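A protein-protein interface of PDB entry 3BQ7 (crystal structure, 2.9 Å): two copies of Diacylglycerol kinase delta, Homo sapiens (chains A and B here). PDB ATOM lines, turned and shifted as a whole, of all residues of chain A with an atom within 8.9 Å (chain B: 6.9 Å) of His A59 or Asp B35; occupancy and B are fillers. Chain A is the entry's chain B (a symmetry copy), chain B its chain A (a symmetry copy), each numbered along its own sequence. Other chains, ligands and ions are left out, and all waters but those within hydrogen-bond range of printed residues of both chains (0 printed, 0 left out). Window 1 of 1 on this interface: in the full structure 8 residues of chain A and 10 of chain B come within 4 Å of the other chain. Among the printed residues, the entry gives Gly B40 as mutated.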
ATOM      1  N   TRP A  18     -10.268 -15.026  22.440  1.00  0.00           N
ATOM      2  CA  TRP A  18     -10.727 -16.238  21.765  1.00  0.00           C
ATOM      3  C   TRP A  18     -10.180 -17.514  22.423  1.00  0.00           C
ATOM      4  O   TRP A  18     -10.946 -18.381  22.849  1.00  0.00           O
ATOM      5  CB  TRP A  18     -10.297 -16.185  20.303  1.00  0.00           C
ATOM      6  CG  TRP A  18     -10.753 -17.341  19.530  1.00  0.00           C
ATOM      7  CD1 TRP A  18     -12.035 -17.655  19.207  1.00  0.00           C
ATOM      8  CD2 TRP A  18      -9.925 -18.371  18.979  1.00  0.00           C
ATOM      9  NE1 TRP A  18     -12.072 -18.819  18.479  1.00  0.00           N
ATOM     10  CE2 TRP A  18     -10.797 -19.278  18.327  1.00  0.00           C
ATOM     11  CE3 TRP A  18      -8.535 -18.610  18.970  1.00  0.00           C
ATOM     12  CZ2 TRP A  18     -10.312 -20.422  17.669  1.00  0.00           C
ATOM     13  CZ3 TRP A  18      -8.061 -19.743  18.314  1.00  0.00           C
ATOM     14  CH2 TRP A  18      -8.952 -20.635  17.670  1.00  0.00           C
ATOM     15  N   LEU A  19      -8.848 -17.608  22.500  1.00  0.00           N
ATOM     16  CA  LEU A  19      -8.172 -18.763  23.099  1.00  0.00           C
ATOM     17  C   LEU A  19      -8.666 -18.980  24.502  1.00  0.00           C
ATOM     18  O   LEU A  19      -8.905 -20.106  24.943  1.00  0.00           O
ATOM     19  CB  LEU A  19      -6.675 -18.534  23.165  1.00  0.00           C
ATOM     20  CG  LEU A  19      -5.903 -18.537  21.859  1.00  0.00           C
ATOM     21  CD1 LEU A  19      -4.449 -18.307  22.185  1.00  0.00           C
ATOM     22  CD2 LEU A  19      -6.080 -19.867  21.143  1.00  0.00           C
ATOM     23  N   LEU A  22     -11.713 -20.551  24.670  1.00  0.00           N
ATOM     24  CA  LEU A  22     -11.645 -21.980  24.396  1.00  0.00           C
ATOM     25  C   LEU A  22     -10.985 -22.652  25.574  1.00  0.00           C
ATOM     26  O   LEU A  22     -10.817 -23.855  25.590  1.00  0.00           O
ATOM     27  CB  LEU A  22     -10.815 -22.235  23.141  1.00  0.00           C
ATOM     28  CG  LEU A  22     -11.263 -21.509  21.868  1.00  0.00           C
ATOM     29  CD1 LEU A  22     -10.437 -22.018  20.709  1.00  0.00           C
ATOM     30  CD2 LEU A  22     -12.737 -21.774  21.600  1.00  0.00           C
ATOM     31  N   SER A  23     -10.625 -21.857  26.569  1.00  0.00           N
ATOM     32  CA  SER A  23      -9.968 -22.397  27.735  1.00  0.00           C
ATOM     33  C   SER A  23      -8.622 -22.904  27.285  1.00  0.00           C
ATOM     34  O   SER A  23      -8.187 -23.975  27.683  1.00  0.00           O
ATOM     35  CB  SER A  23     -10.768 -23.542  28.335  1.00  0.00           C
ATOM     36  OG  SER A  23     -11.993 -23.077  28.852  1.00  0.00           O
ATOM     37  N   LEU A  24      -7.980 -22.146  26.411  1.00  0.00           N
ATOM     38  CA  LEU A  24      -6.667 -22.517  25.949  1.00  0.00           C
ATOM     39  C   LEU A  24      -5.776 -21.328  26.277  1.00  0.00           C
ATOM     40  O   LEU A  24      -4.838 -21.012  25.561  1.00  0.00           O
ATOM     41  CB  LEU A  24      -6.694 -22.791  24.452  1.00  0.00           C
ATOM     42  CG  LEU A  24      -7.529 -23.983  23.999  1.00  0.00           C
ATOM     43  CD1 LEU A  24      -7.453 -24.156  22.483  1.00  0.00           C
ATOM     44  CD2 LEU A  24      -7.008 -25.229  24.668  1.00  0.00           C
ATOM     45  N   CYS A  25      -6.078 -20.681  27.392  1.00  0.00           N
ATOM     46  CA  CYS A  25      -5.325 -19.510  27.847  1.00  0.00           C
ATOM     47  C   CYS A  25      -3.833 -19.771  27.943  1.00  0.00           C
ATOM     48  O   CYS A  25      -3.019 -18.856  27.765  1.00  0.00           O
ATOM     49  CB  CYS A  25      -5.818 -19.078  29.222  1.00  0.00           C
ATOM     50  SG  CYS A  25      -7.602 -19.040  29.341  1.00  0.00           S
ATOM     51  N   GLU A  26      -3.496 -21.017  28.257  1.00  0.00           N
ATOM     52  CA  GLU A  26      -2.115 -21.444  28.400  1.00  0.00           C
ATOM     53  C   GLU A  26      -1.329 -21.279  27.116  1.00  0.00           C
ATOM     54  O   GLU A  26      -0.134 -21.578  27.084  1.00  0.00           O
ATOM     55  N   TYR A  27      -1.986 -20.806  26.058  1.00  0.00           N
ATOM     56  CA  TYR A  27      -1.311 -20.593  24.773  1.00  0.00           C
ATOM     57  C   TYR A  27      -1.287 -19.112  24.396  1.00  0.00           C
ATOM     58  O   TYR A  27      -0.625 -18.736  23.432  1.00  0.00           O
ATOM     59  CB  TYR A  27      -2.007 -21.384  23.643  1.00  0.00           C
ATOM     60  CG  TYR A  27      -1.920 -22.892  23.764  1.00  0.00           C
ATOM     61  CD1 TYR A  27      -2.984 -23.642  24.261  1.00  0.00           C
ATOM     62  CD2 TYR A  27      -0.767 -23.562  23.391  1.00  0.00           C
ATOM     63  CE1 TYR A  27      -2.899 -25.011  24.379  1.00  0.00           C
ATOM     64  CE2 TYR A  27      -0.670 -24.927  23.510  1.00  0.00           C
ATOM     65  CZ  TYR A  27      -1.739 -25.650  24.006  1.00  0.00           C
ATOM     66  OH  TYR A  27      -1.632 -27.016  24.124  1.00  0.00           O
ATOM     67  N   PHE A  31       0.962 -17.339  21.054  1.00  0.00           N
ATOM     68  CA  PHE A  31       0.051 -16.749  20.072  1.00  0.00           C
ATOM     69  C   PHE A  31       0.193 -15.257  20.006  1.00  0.00           C
ATOM     70  O   PHE A  31      -0.155 -14.611  19.013  1.00  0.00           O
ATOM     71  CB  PHE A  31      -1.404 -17.093  20.360  1.00  0.00           C
ATOM     72  CG  PHE A  31      -1.847 -18.362  19.719  1.00  0.00           C
ATOM     73  CD1 PHE A  31      -1.269 -19.575  20.089  1.00  0.00           C
ATOM     74  CD2 PHE A  31      -2.789 -18.341  18.702  1.00  0.00           C
ATOM     75  CE1 PHE A  31      -1.636 -20.754  19.471  1.00  0.00           C
ATOM     76  CE2 PHE A  31      -3.168 -19.505  18.075  1.00  0.00           C
ATOM     77  CZ  PHE A  31      -2.581 -20.722  18.451  1.00  0.00           C
ATOM     78  N   LEU A  49       0.592 -24.846  14.108  1.00  0.00           N
ATOM     79  CA  LEU A  49       0.318 -25.119  15.517  1.00  0.00           C
ATOM     80  C   LEU A  49       1.483 -25.861  16.123  1.00  0.00           C
ATOM     81  O   LEU A  49       1.851 -25.592  17.247  1.00  0.00           O
ATOM     82  CB  LEU A  49      -0.936 -25.960  15.649  1.00  0.00           C
ATOM     83  CG  LEU A  49      -2.165 -25.345  14.987  1.00  0.00           C
ATOM     84  CD1 LEU A  49      -3.341 -26.223  15.251  1.00  0.00           C
ATOM     85  CD2 LEU A  49      -2.421 -23.939  15.516  1.00  0.00           C
ATOM     86  N   GLY A  53       3.906 -24.346  19.033  1.00  0.00           N
ATOM     87  CA  GLY A  53       3.997 -24.952  20.342  1.00  0.00           C
ATOM     88  C   GLY A  53       2.889 -25.912  20.730  1.00  0.00           C
ATOM     89  O   GLY A  53       3.118 -26.762  21.588  1.00  0.00           O
ATOM     90  N   VAL A  54       1.702 -25.787  20.136  1.00  0.00           N
ATOM     91  CA  VAL A  54       0.603 -26.693  20.466  1.00  0.00           C
ATOM     92  C   VAL A  54       0.952 -28.135  20.095  1.00  0.00           C
ATOM     93  O   VAL A  54       1.478 -28.377  19.023  1.00  0.00           O
ATOM     94  CB  VAL A  54      -0.689 -26.304  19.726  1.00  0.00           C
ATOM     95  CG1 VAL A  54      -1.848 -27.208  20.196  1.00  0.00           C
ATOM     96  CG2 VAL A  54      -1.010 -24.831  19.978  1.00  0.00           C
ATOM     97  N   THR A  55       0.660 -29.092  20.975  1.00  0.00           N
ATOM     98  CA  THR A  55       0.979 -30.500  20.707  1.00  0.00           C
ATOM     99  C   THR A  55      -0.120 -31.468  21.079  1.00  0.00           C
ATOM    100  O   THR A  55      -0.298 -32.470  20.416  1.00  0.00           O
ATOM    101  CB  THR A  55       2.261 -30.972  21.443  1.00  0.00           C
ATOM    102  OG1 THR A  55       2.148 -30.724  22.850  1.00  0.00           O
ATOM    103  CG2 THR A  55       3.477 -30.263  20.887  1.00  0.00           C
ATOM    104  N   LYS A  56      -0.836 -31.213  22.158  1.00  0.00           N
ATOM    105  CA  LYS A  56      -1.901 -32.126  22.502  1.00  0.00           C
ATOM    106  C   LYS A  56      -2.933 -32.016  21.396  1.00  0.00           C
ATOM    107  O   LYS A  56      -3.622 -30.998  21.260  1.00  0.00           O
ATOM    108  N   VAL A  57      -3.016 -33.072  20.598  1.00  0.00           N
ATOM    109  CA  VAL A  57      -3.931 -33.131  19.482  1.00  0.00           C
ATOM    110  C   VAL A  57      -5.246 -32.503  19.831  1.00  0.00           C
ATOM    111  O   VAL A  57      -5.692 -31.590  19.139  1.00  0.00           O
ATOM    112  CB  VAL A  57      -4.169 -34.565  19.061  1.00  0.00           C
ATOM    113  CG1 VAL A  57      -5.230 -34.608  18.038  1.00  0.00           C
ATOM    114  CG2 VAL A  57      -2.903 -35.158  18.488  1.00  0.00           C
ATOM    115  N   GLY A  58      -5.863 -32.996  20.904  1.00  0.00           N
ATOM    116  CA  GLY A  58      -7.145 -32.466  21.343  1.00  0.00           C
ATOM    117  C   GLY A  58      -7.178 -30.949  21.367  1.00  0.00           C
ATOM    118  O   GLY A  58      -8.245 -30.345  21.375  1.00  0.00           O
ATOM    119  N   HIS A  59      -6.000 -30.337  21.399  1.00  0.00           N
ATOM    120  CA  HIS A  59      -5.898 -28.882  21.407  1.00  0.00           C
ATOM    121  C   HIS A  59      -5.745 -28.349  20.008  1.00  0.00           C
ATOM    122  O   HIS A  59      -6.391 -27.357  19.675  1.00  0.00           O
ATOM    123  CB  HIS A  59      -4.736 -28.431  22.269  1.00  0.00           C
ATOM    124  CG  HIS A  59      -4.954 -28.718  23.710  1.00  0.00           C
ATOM    125  ND1 HIS A  59      -4.049 -28.396  24.692  1.00  0.00           N
ATOM    126  CD2 HIS A  59      -5.991 -29.335  24.341  1.00  0.00           C
ATOM    127  CE1 HIS A  59      -4.509 -28.799  25.867  1.00  0.00           C
ATOM    128  NE2 HIS A  59      -5.688 -29.372  25.676  1.00  0.00           N
ATOM    129  N   MET A  60      -4.870 -28.977  19.212  1.00  0.00           N
ATOM    130  CA  MET A  60      -4.736 -28.539  17.835  1.00  0.00           C
ATOM    131  C   MET A  60      -6.132 -28.580  17.213  1.00  0.00           C
ATOM    132  O   MET A  60      -6.598 -27.632  16.622  1.00  0.00           O
ATOM    133  CB  MET A  60      -3.806 -29.467  17.055  1.00  0.00           C
ATOM    134  CG  MET A  60      -2.352 -29.360  17.472  1.00  0.00           C
ATOM    135  SD  MET A  60      -1.309 -30.287  16.388  1.00  0.00           S
ATOM    136  CE  MET A  60      -1.532 -31.921  16.944  1.00  0.00           C
ATOM    137  N   LYS A  61      -6.814 -29.699  17.446  1.00  0.00           N
ATOM    138  CA  LYS A  61      -8.176 -29.847  16.949  1.00  0.00           C
ATOM    139  C   LYS A  61      -9.070 -28.764  17.532  1.00  0.00           C
ATOM    140  O   LYS A  61      -9.793 -28.105  16.799  1.00  0.00           O
ATOM    141  CB  LYS A  61      -8.711 -31.196  17.317  1.00  0.00           C
ATOM    142  CG  LYS A  61      -8.039 -32.277  16.569  1.00  0.00           C
ATOM    143  CD  LYS A  61      -8.611 -33.544  16.964  1.00  0.00           C
ATOM    144  CE  LYS A  61      -7.962 -34.671  16.273  1.00  0.00           C
ATOM    145  NZ  LYS A  61      -8.740 -35.847  16.748  1.00  0.00           N
ATOM    146  N   ARG A  62      -9.026 -28.600  18.851  1.00  0.00           N
ATOM    147  CA  ARG A  62      -9.868 -27.591  19.478  1.00  0.00           C
ATOM    148  C   ARG A  62      -9.662 -26.213  18.860  1.00  0.00           C
ATOM    149  O   ARG A  62     -10.597 -25.455  18.677  1.00  0.00           O
ATOM    150  CB  ARG A  62      -9.589 -27.487  20.962  1.00  0.00           C
ATOM    151  CG  ARG A  62     -10.522 -26.497  21.637  1.00  0.00           C
ATOM    152  CD  ARG A  62     -10.244 -26.368  23.122  1.00  0.00           C
ATOM    153  NE  ARG A  62     -10.188 -27.674  23.779  1.00  0.00           N
ATOM    154  CZ  ARG A  62     -10.042 -27.844  25.089  1.00  0.00           C
ATOM    155  NH1 ARG A  62      -9.944 -26.780  25.880  1.00  0.00           N
ATOM    156  NH2 ARG A  62      -9.971 -29.071  25.597  1.00  0.00           N
ATOM    157  N   ILE A  63      -8.418 -25.884  18.560  1.00  0.00           N
ATOM    158  CA  ILE A  63      -8.098 -24.593  17.965  1.00  0.00           C
ATOM    159  C   ILE A  63      -8.540 -24.583  16.521  1.00  0.00           C
ATOM    160  O   ILE A  63      -9.200 -23.666  16.099  1.00  0.00           O
ATOM    161  CB  ILE A  63      -6.581 -24.316  17.973  1.00  0.00           C
ATOM    162  CG1 ILE A  63      -6.053 -24.279  19.411  1.00  0.00           C
ATOM    163  CG2 ILE A  63      -6.290 -23.009  17.284  1.00  0.00           C
ATOM    164  CD1 ILE A  63      -4.548 -24.253  19.490  1.00  0.00           C
ATOM    165  N   LEU A  64      -8.165 -25.607  15.766  1.00  0.00           N
ATOM    166  CA  LEU A  64      -8.515 -25.702  14.358  1.00  0.00           C
ATOM    167  C   LEU A  64     -10.011 -25.647  14.104  1.00  0.00           C
ATOM    168  O   LEU A  64     -10.461 -25.000  13.161  1.00  0.00           O
ATOM    169  CB  LEU A  64      -7.945 -26.989  13.766  1.00  0.00           C
ATOM    170  CG  LEU A  64      -6.421 -27.105  13.871  1.00  0.00           C
ATOM    171  CD1 LEU A  64      -5.971 -28.462  13.376  1.00  0.00           C
ATOM    172  CD2 LEU A  64      -5.761 -26.008  13.082  1.00  0.00           C
ATOM    173  N   CYS A  65     -10.790 -26.321  14.940  1.00  0.00           N
ATOM    174  CA  CYS A  65     -12.231 -26.323  14.758  1.00  0.00           C
ATOM    175  C   CYS A  65     -12.807 -25.007  15.236  1.00  0.00           C
ATOM    176  O   CYS A  65     -13.833 -24.552  14.731  1.00  0.00           O
ATOM    177  CB  CYS A  65     -12.864 -27.505  15.501  1.00  0.00           C
ATOM    178  SG  CYS A  65     -12.428 -29.153  14.756  1.00  0.00           S
ATOM    179  N   GLY A  66     -12.135 -24.390  16.201  1.00  0.00           N
ATOM    180  CA  GLY A  66     -12.594 -23.111  16.708  1.00  0.00           C
ATOM    181  C   GLY A  66     -12.471 -22.093  15.590  1.00  0.00           C
ATOM    182  O   GLY A  66     -13.110 -21.043  15.651  1.00  0.00           O
ATOM    183  N   ILE A  67     -11.652 -22.433  14.581  1.00  0.00           N
ATOM    184  CA  ILE A  67     -11.391 -21.605  13.391  1.00  0.00           C
ATOM    185  C   ILE A  67     -12.442 -21.902  12.332  1.00  0.00           C
ATOM    186  O   ILE A  67     -13.108 -21.001  11.845  1.00  0.00           O
ATOM    187  CB  ILE A  67     -10.010 -21.899  12.741  1.00  0.00           C
ATOM    188  CG1 ILE A  67      -8.855 -21.553  13.700  1.00  0.00           C
ATOM    189  CG2 ILE A  67      -9.883 -21.118  11.459  1.00  0.00           C
ATOM    190  CD1 ILE A  67      -8.730 -20.101  14.015  1.00  0.00           C
ATOM    191  N   GLY B  11     -15.945 -36.174  28.511  1.00  0.00           N
ATOM    192  CA  GLY B  11     -14.778 -35.621  29.146  1.00  0.00           C
ATOM    193  C   GLY B  11     -13.670 -36.569  28.717  1.00  0.00           C
ATOM    194  O   GLY B  11     -13.926 -37.635  28.132  1.00  0.00           O
ATOM    195  N   THR B  12     -12.430 -36.203  29.000  1.00  0.00           N
ATOM    196  CA  THR B  12     -11.295 -37.046  28.623  1.00  0.00           C
ATOM    197  C   THR B  12     -11.415 -38.489  29.132  1.00  0.00           C
ATOM    198  O   THR B  12     -10.925 -39.434  28.511  1.00  0.00           O
ATOM    199  CB  THR B  12      -9.992 -36.470  29.174  1.00  0.00           C
ATOM    200  OG1 THR B  12      -8.888 -37.221  28.656  1.00  0.00           O
ATOM    201  CG2 THR B  12      -9.989 -36.549  30.695  1.00  0.00           C
ATOM    202  N   ASP B  29      -3.694 -43.733  27.604  1.00  0.00           N
ATOM    203  CA  ASP B  29      -2.698 -42.740  28.032  1.00  0.00           C
ATOM    204  C   ASP B  29      -2.649 -41.503  27.182  1.00  0.00           C
ATOM    205  O   ASP B  29      -3.095 -40.442  27.577  1.00  0.00           O
ATOM    206  CB  ASP B  29      -1.323 -43.344  28.009  1.00  0.00           C
ATOM    207  CG  ASP B  29      -1.154 -44.350  29.081  1.00  0.00           C
ATOM    208  OD1 ASP B  29      -1.788 -45.426  28.976  1.00  0.00           O
ATOM    209  OD2 ASP B  29      -0.417 -44.051  30.042  1.00  0.00           O
ATOM    210  N   ILE B  30      -2.035 -41.646  26.023  1.00  0.00           N
ATOM    211  CA  ILE B  30      -1.923 -40.551  25.099  1.00  0.00           C
ATOM    212  C   ILE B  30      -3.244 -39.876  24.879  1.00  0.00           C
ATOM    213  O   ILE B  30      -3.328 -38.662  24.938  1.00  0.00           O
ATOM    214  CB  ILE B  30      -1.451 -41.041  23.773  1.00  0.00           C
ATOM    215  CG1 ILE B  30      -1.871 -42.505  23.622  1.00  0.00           C
ATOM    216  CG2 ILE B  30       0.037 -40.838  23.664  1.00  0.00           C
ATOM    217  CD1 ILE B  30      -1.184 -43.235  22.508  1.00  0.00           C
ATOM    218  N   PHE B  31      -4.282 -40.660  24.614  1.00  0.00           N
ATOM    219  CA  PHE B  31      -5.591 -40.076  24.364  1.00  0.00           C
ATOM    220  C   PHE B  31      -6.008 -39.177  25.494  1.00  0.00           C
ATOM    221  O   PHE B  31      -6.844 -38.284  25.337  1.00  0.00           O
ATOM    222  CB  PHE B  31      -6.649 -41.154  24.151  1.00  0.00           C
ATOM    223  CG  PHE B  31      -6.800 -41.579  22.729  1.00  0.00           C
ATOM    224  CD1 PHE B  31      -5.766 -42.215  22.076  1.00  0.00           C
ATOM    225  CD2 PHE B  31      -7.954 -41.278  22.026  1.00  0.00           C
ATOM    226  CE1 PHE B  31      -5.883 -42.575  20.775  1.00  0.00           C
ATOM    227  CE2 PHE B  31      -8.086 -41.638  20.709  1.00  0.00           C
ATOM    228  CZ  PHE B  31      -7.035 -42.276  20.075  1.00  0.00           C
ATOM    229  N   THR B  32      -5.406 -39.424  26.643  1.00  0.00           N
ATOM    230  CA  THR B  32      -5.707 -38.643  27.809  1.00  0.00           C
ATOM    231  C   THR B  32      -4.761 -37.479  27.845  1.00  0.00           C
ATOM    232  O   THR B  32      -5.189 -36.351  28.067  1.00  0.00           O
ATOM    233  CB  THR B  32      -5.575 -39.467  29.083  1.00  0.00           C
ATOM    234  OG1 THR B  32      -6.706 -40.346  29.194  1.00  0.00           O
ATOM    235  CG2 THR B  32      -5.528 -38.554  30.295  1.00  0.00           C
ATOM    236  N   ARG B  33      -3.480 -37.732  27.632  1.00  0.00           N
ATOM    237  CA  ARG B  33      -2.530 -36.629  27.627  1.00  0.00           C
ATOM    238  C   ARG B  33      -2.896 -35.551  26.602  1.00  0.00           C
ATOM    239  O   ARG B  33      -2.928 -34.361  26.917  1.00  0.00           O
ATOM    240  CB  ARG B  33      -1.126 -37.127  27.277  1.00  0.00           C
ATOM    241  CG  ARG B  33      -0.640 -38.229  28.157  1.00  0.00           C
ATOM    242  CD  ARG B  33       0.568 -38.898  27.538  1.00  0.00           C
ATOM    243  NE  ARG B  33       0.710 -40.269  28.017  1.00  0.00           N
ATOM    244  CZ  ARG B  33       1.595 -41.142  27.548  1.00  0.00           C
ATOM    245  NH1 ARG B  33       2.429 -40.758  26.563  1.00  0.00           N
ATOM    246  NH2 ARG B  33       1.633 -42.386  28.073  1.00  0.00           N
ATOM    247  N   HIS B  34      -3.227 -35.970  25.389  1.00  0.00           N
ATOM    248  CA  HIS B  34      -3.577 -35.012  24.364  1.00  0.00           C
ATOM    249  C   HIS B  34      -4.967 -34.405  24.580  1.00  0.00           C
ATOM    250  O   HIS B  34      -5.567 -33.834  23.659  1.00  0.00           O
ATOM    251  CB  HIS B  34      -3.484 -35.650  22.990  1.00  0.00           C
ATOM    252  CG  HIS B  34      -2.098 -36.062  22.615  1.00  0.00           C
ATOM    253  ND1 HIS B  34      -1.453 -37.126  23.211  1.00  0.00           N
ATOM    254  CD2 HIS B  34      -1.220 -35.536  21.733  1.00  0.00           C
ATOM    255  CE1 HIS B  34      -0.236 -37.230  22.713  1.00  0.00           C
ATOM    256  NE2 HIS B  34      -0.067 -36.278  21.815  1.00  0.00           N
ATOM    257  N   ASP B  35      -5.480 -34.541  25.798  1.00  0.00           N
ATOM    258  CA  ASP B  35      -6.769 -33.960  26.140  1.00  0.00           C
ATOM    259  C   ASP B  35      -7.775 -34.188  25.032  1.00  0.00           C
ATOM    260  O   ASP B  35      -8.443 -33.247  24.564  1.00  0.00           O
ATOM    261  CB  ASP B  35      -6.600 -32.471  26.342  1.00  0.00           C
ATOM    262  CG  ASP B  35      -7.738 -31.869  27.032  1.00  0.00           C
ATOM    263  OD1 ASP B  35      -7.763 -30.667  27.152  1.00  0.00           O
ATOM    264  OD2 ASP B  35      -8.621 -32.575  27.480  1.00  0.00           O
ATOM    265  N   ILE B  36      -7.864 -35.442  24.609  1.00  0.00           N
ATOM    266  CA  ILE B  36      -8.773 -35.825  23.548  1.00  0.00           C
ATOM    267  C   ILE B  36     -10.212 -35.810  24.075  1.00  0.00           C
ATOM    268  O   ILE B  36     -10.709 -36.829  24.585  1.00  0.00           O
ATOM    269  CB  ILE B  36      -8.426 -37.234  23.029  1.00  0.00           C
ATOM    270  CG1 ILE B  36      -6.964 -37.280  22.587  1.00  0.00           C
ATOM    271  CG2 ILE B  36      -9.324 -37.585  21.858  1.00  0.00           C
ATOM    272  CD1 ILE B  36      -6.654 -36.345  21.424  1.00  0.00           C
ATOM    273  N   ARG B  37     -10.872 -34.656  23.969  1.00  0.00           N
ATOM    274  CA  ARG B  37     -12.259 -34.533  24.428  1.00  0.00           C
ATOM    275  C   ARG B  37     -13.212 -35.289  23.509  1.00  0.00           C
ATOM    276  O   ARG B  37     -12.815 -35.781  22.455  1.00  0.00           O
ATOM    277  CB  ARG B  37     -12.687 -33.066  24.481  1.00  0.00           C
ATOM    278  CG  ARG B  37     -12.043 -32.297  25.600  1.00  0.00           C
ATOM    279  CD  ARG B  37     -12.388 -32.910  26.949  1.00  0.00           C
ATOM    280  NE  ARG B  37     -11.628 -32.287  28.037  1.00  0.00           N
ATOM    281  CZ  ARG B  37     -11.673 -30.991  28.335  1.00  0.00           C
ATOM    282  NH1 ARG B  37     -12.447 -30.183  27.628  1.00  0.00           N
ATOM    283  NH2 ARG B  37     -10.940 -30.496  29.328  1.00  0.00           N
ATOM    284  N   GLY B  38     -14.478 -35.361  23.899  1.00  0.00           N
ATOM    285  CA  GLY B  38     -15.435 -36.076  23.083  1.00  0.00           C
ATOM    286  C   GLY B  38     -15.319 -35.656  21.640  1.00  0.00           C
ATOM    287  O   GLY B  38     -14.856 -36.409  20.779  1.00  0.00           O
ATOM    288  N   GLY B  40     -13.248 -33.902  19.898  1.00  0.00           N
ATOM    289  CA  GLY B  40     -11.981 -34.162  19.240  1.00  0.00           C
ATOM    290  C   GLY B  40     -12.025 -35.488  18.499  1.00  0.00           C
ATOM    291  O   GLY B  40     -11.742 -35.549  17.310  1.00  0.00           O
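The guanidinium group (NH2) of Arg A62 sits close to the guanidinium group (NH1) of Arg B37, at 3.4 Å. O of His B34 is in hydrogen-bond range of N of Gly A58, at 2.9 Å. OD1 of Asp B35 is in salt-bridge range of NH2 of Arg A62 (3.1 Å). The side-chain carboxylate (OD1) of Asp B35 is in hydrogen-bond range of a ring nitrogen (NE2) of His A59, 2.9 Å away. O of Gly B40 is in hydrogen-bond range of NZ of Lys A61.
O of Lys A61 lies close to SG of Cys A65, at 3.5 Å. The backbone carbonyl oxygen (O) of Ile B30 lies within hydrogen-bond range of a ring nitrogen (ND1) of His B34. N of Ile B36 lies close to O of Phe B31. The guanidinium group of Arg A62 is in hydrogen-bond range of the backbone carbonyl oxygen of Leu A22, at 3.1 Å. The side-chain carboxylate of Asp B35 is in salt-bridge range of the guanidinium group of Arg B37 (3.1 Å). The side-chain hydroxyl of Tyr A27 lies within hydrogen-bond range of a ring nitrogen (ND1) of His A59 (2.8 Å).
Among the printed residues, pairs that only touch across the chains: Thr A55 with His B34 (3.5 Å), Lys A56 with His B34 (3.6 Å), Val A57 with His B34 (3.3 Å), Val A57 with Ile B36 (3.9 Å), Gly A58 with Asp B35 (3.6 Å) and Gly A58 with Ile B36 (3.5 Å).
His A59 touches one residue of chain B. Of chain B, only His B34, Asp B35 and Ile B36 come within 4 Å of Gly A58. Of the printed residues of chain A, His B34 touches Thr A55 (3.5 Å), Lys A56 (3.6 Å), Val A57 (3.3 Å) and Gly A58 (2.9 Å). Of the printed residues of chain B, Lys A61 touches Gly B40 (3.1 Å). Of the printed residues of chain B, Lys A56 touches His B34. Of the printed residues of chain A, Gly B40 touches Lys A61. Of the printed residues of chain B, Val A57 touches His B34 (3.3 Å) and Ile B36 (3.9 Å). Ser A23 touches none of the printed residues of chain B. Glu A26 touches none of the printed residues of chain B. The nearest printed residue of chain A that does not touch Gly B40 is Gly A58 (5.5 Å).
Printed residues of chain B that touch a printed residue of chain A: His B34, Asp B35, Ile B36, Arg B37 and Gly B40. Hydrophobic or aromatic side chains of chain B that line the printed part of chain A: His B34 and Ile B36. Of the 25 printed residues of chain A, 7 touch a printed residue of chain B.
Position printed for both chains: 31. Of the 11 pairs that touch across the chains among the printed residues, none has its exchanged pair printed and touching as well.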
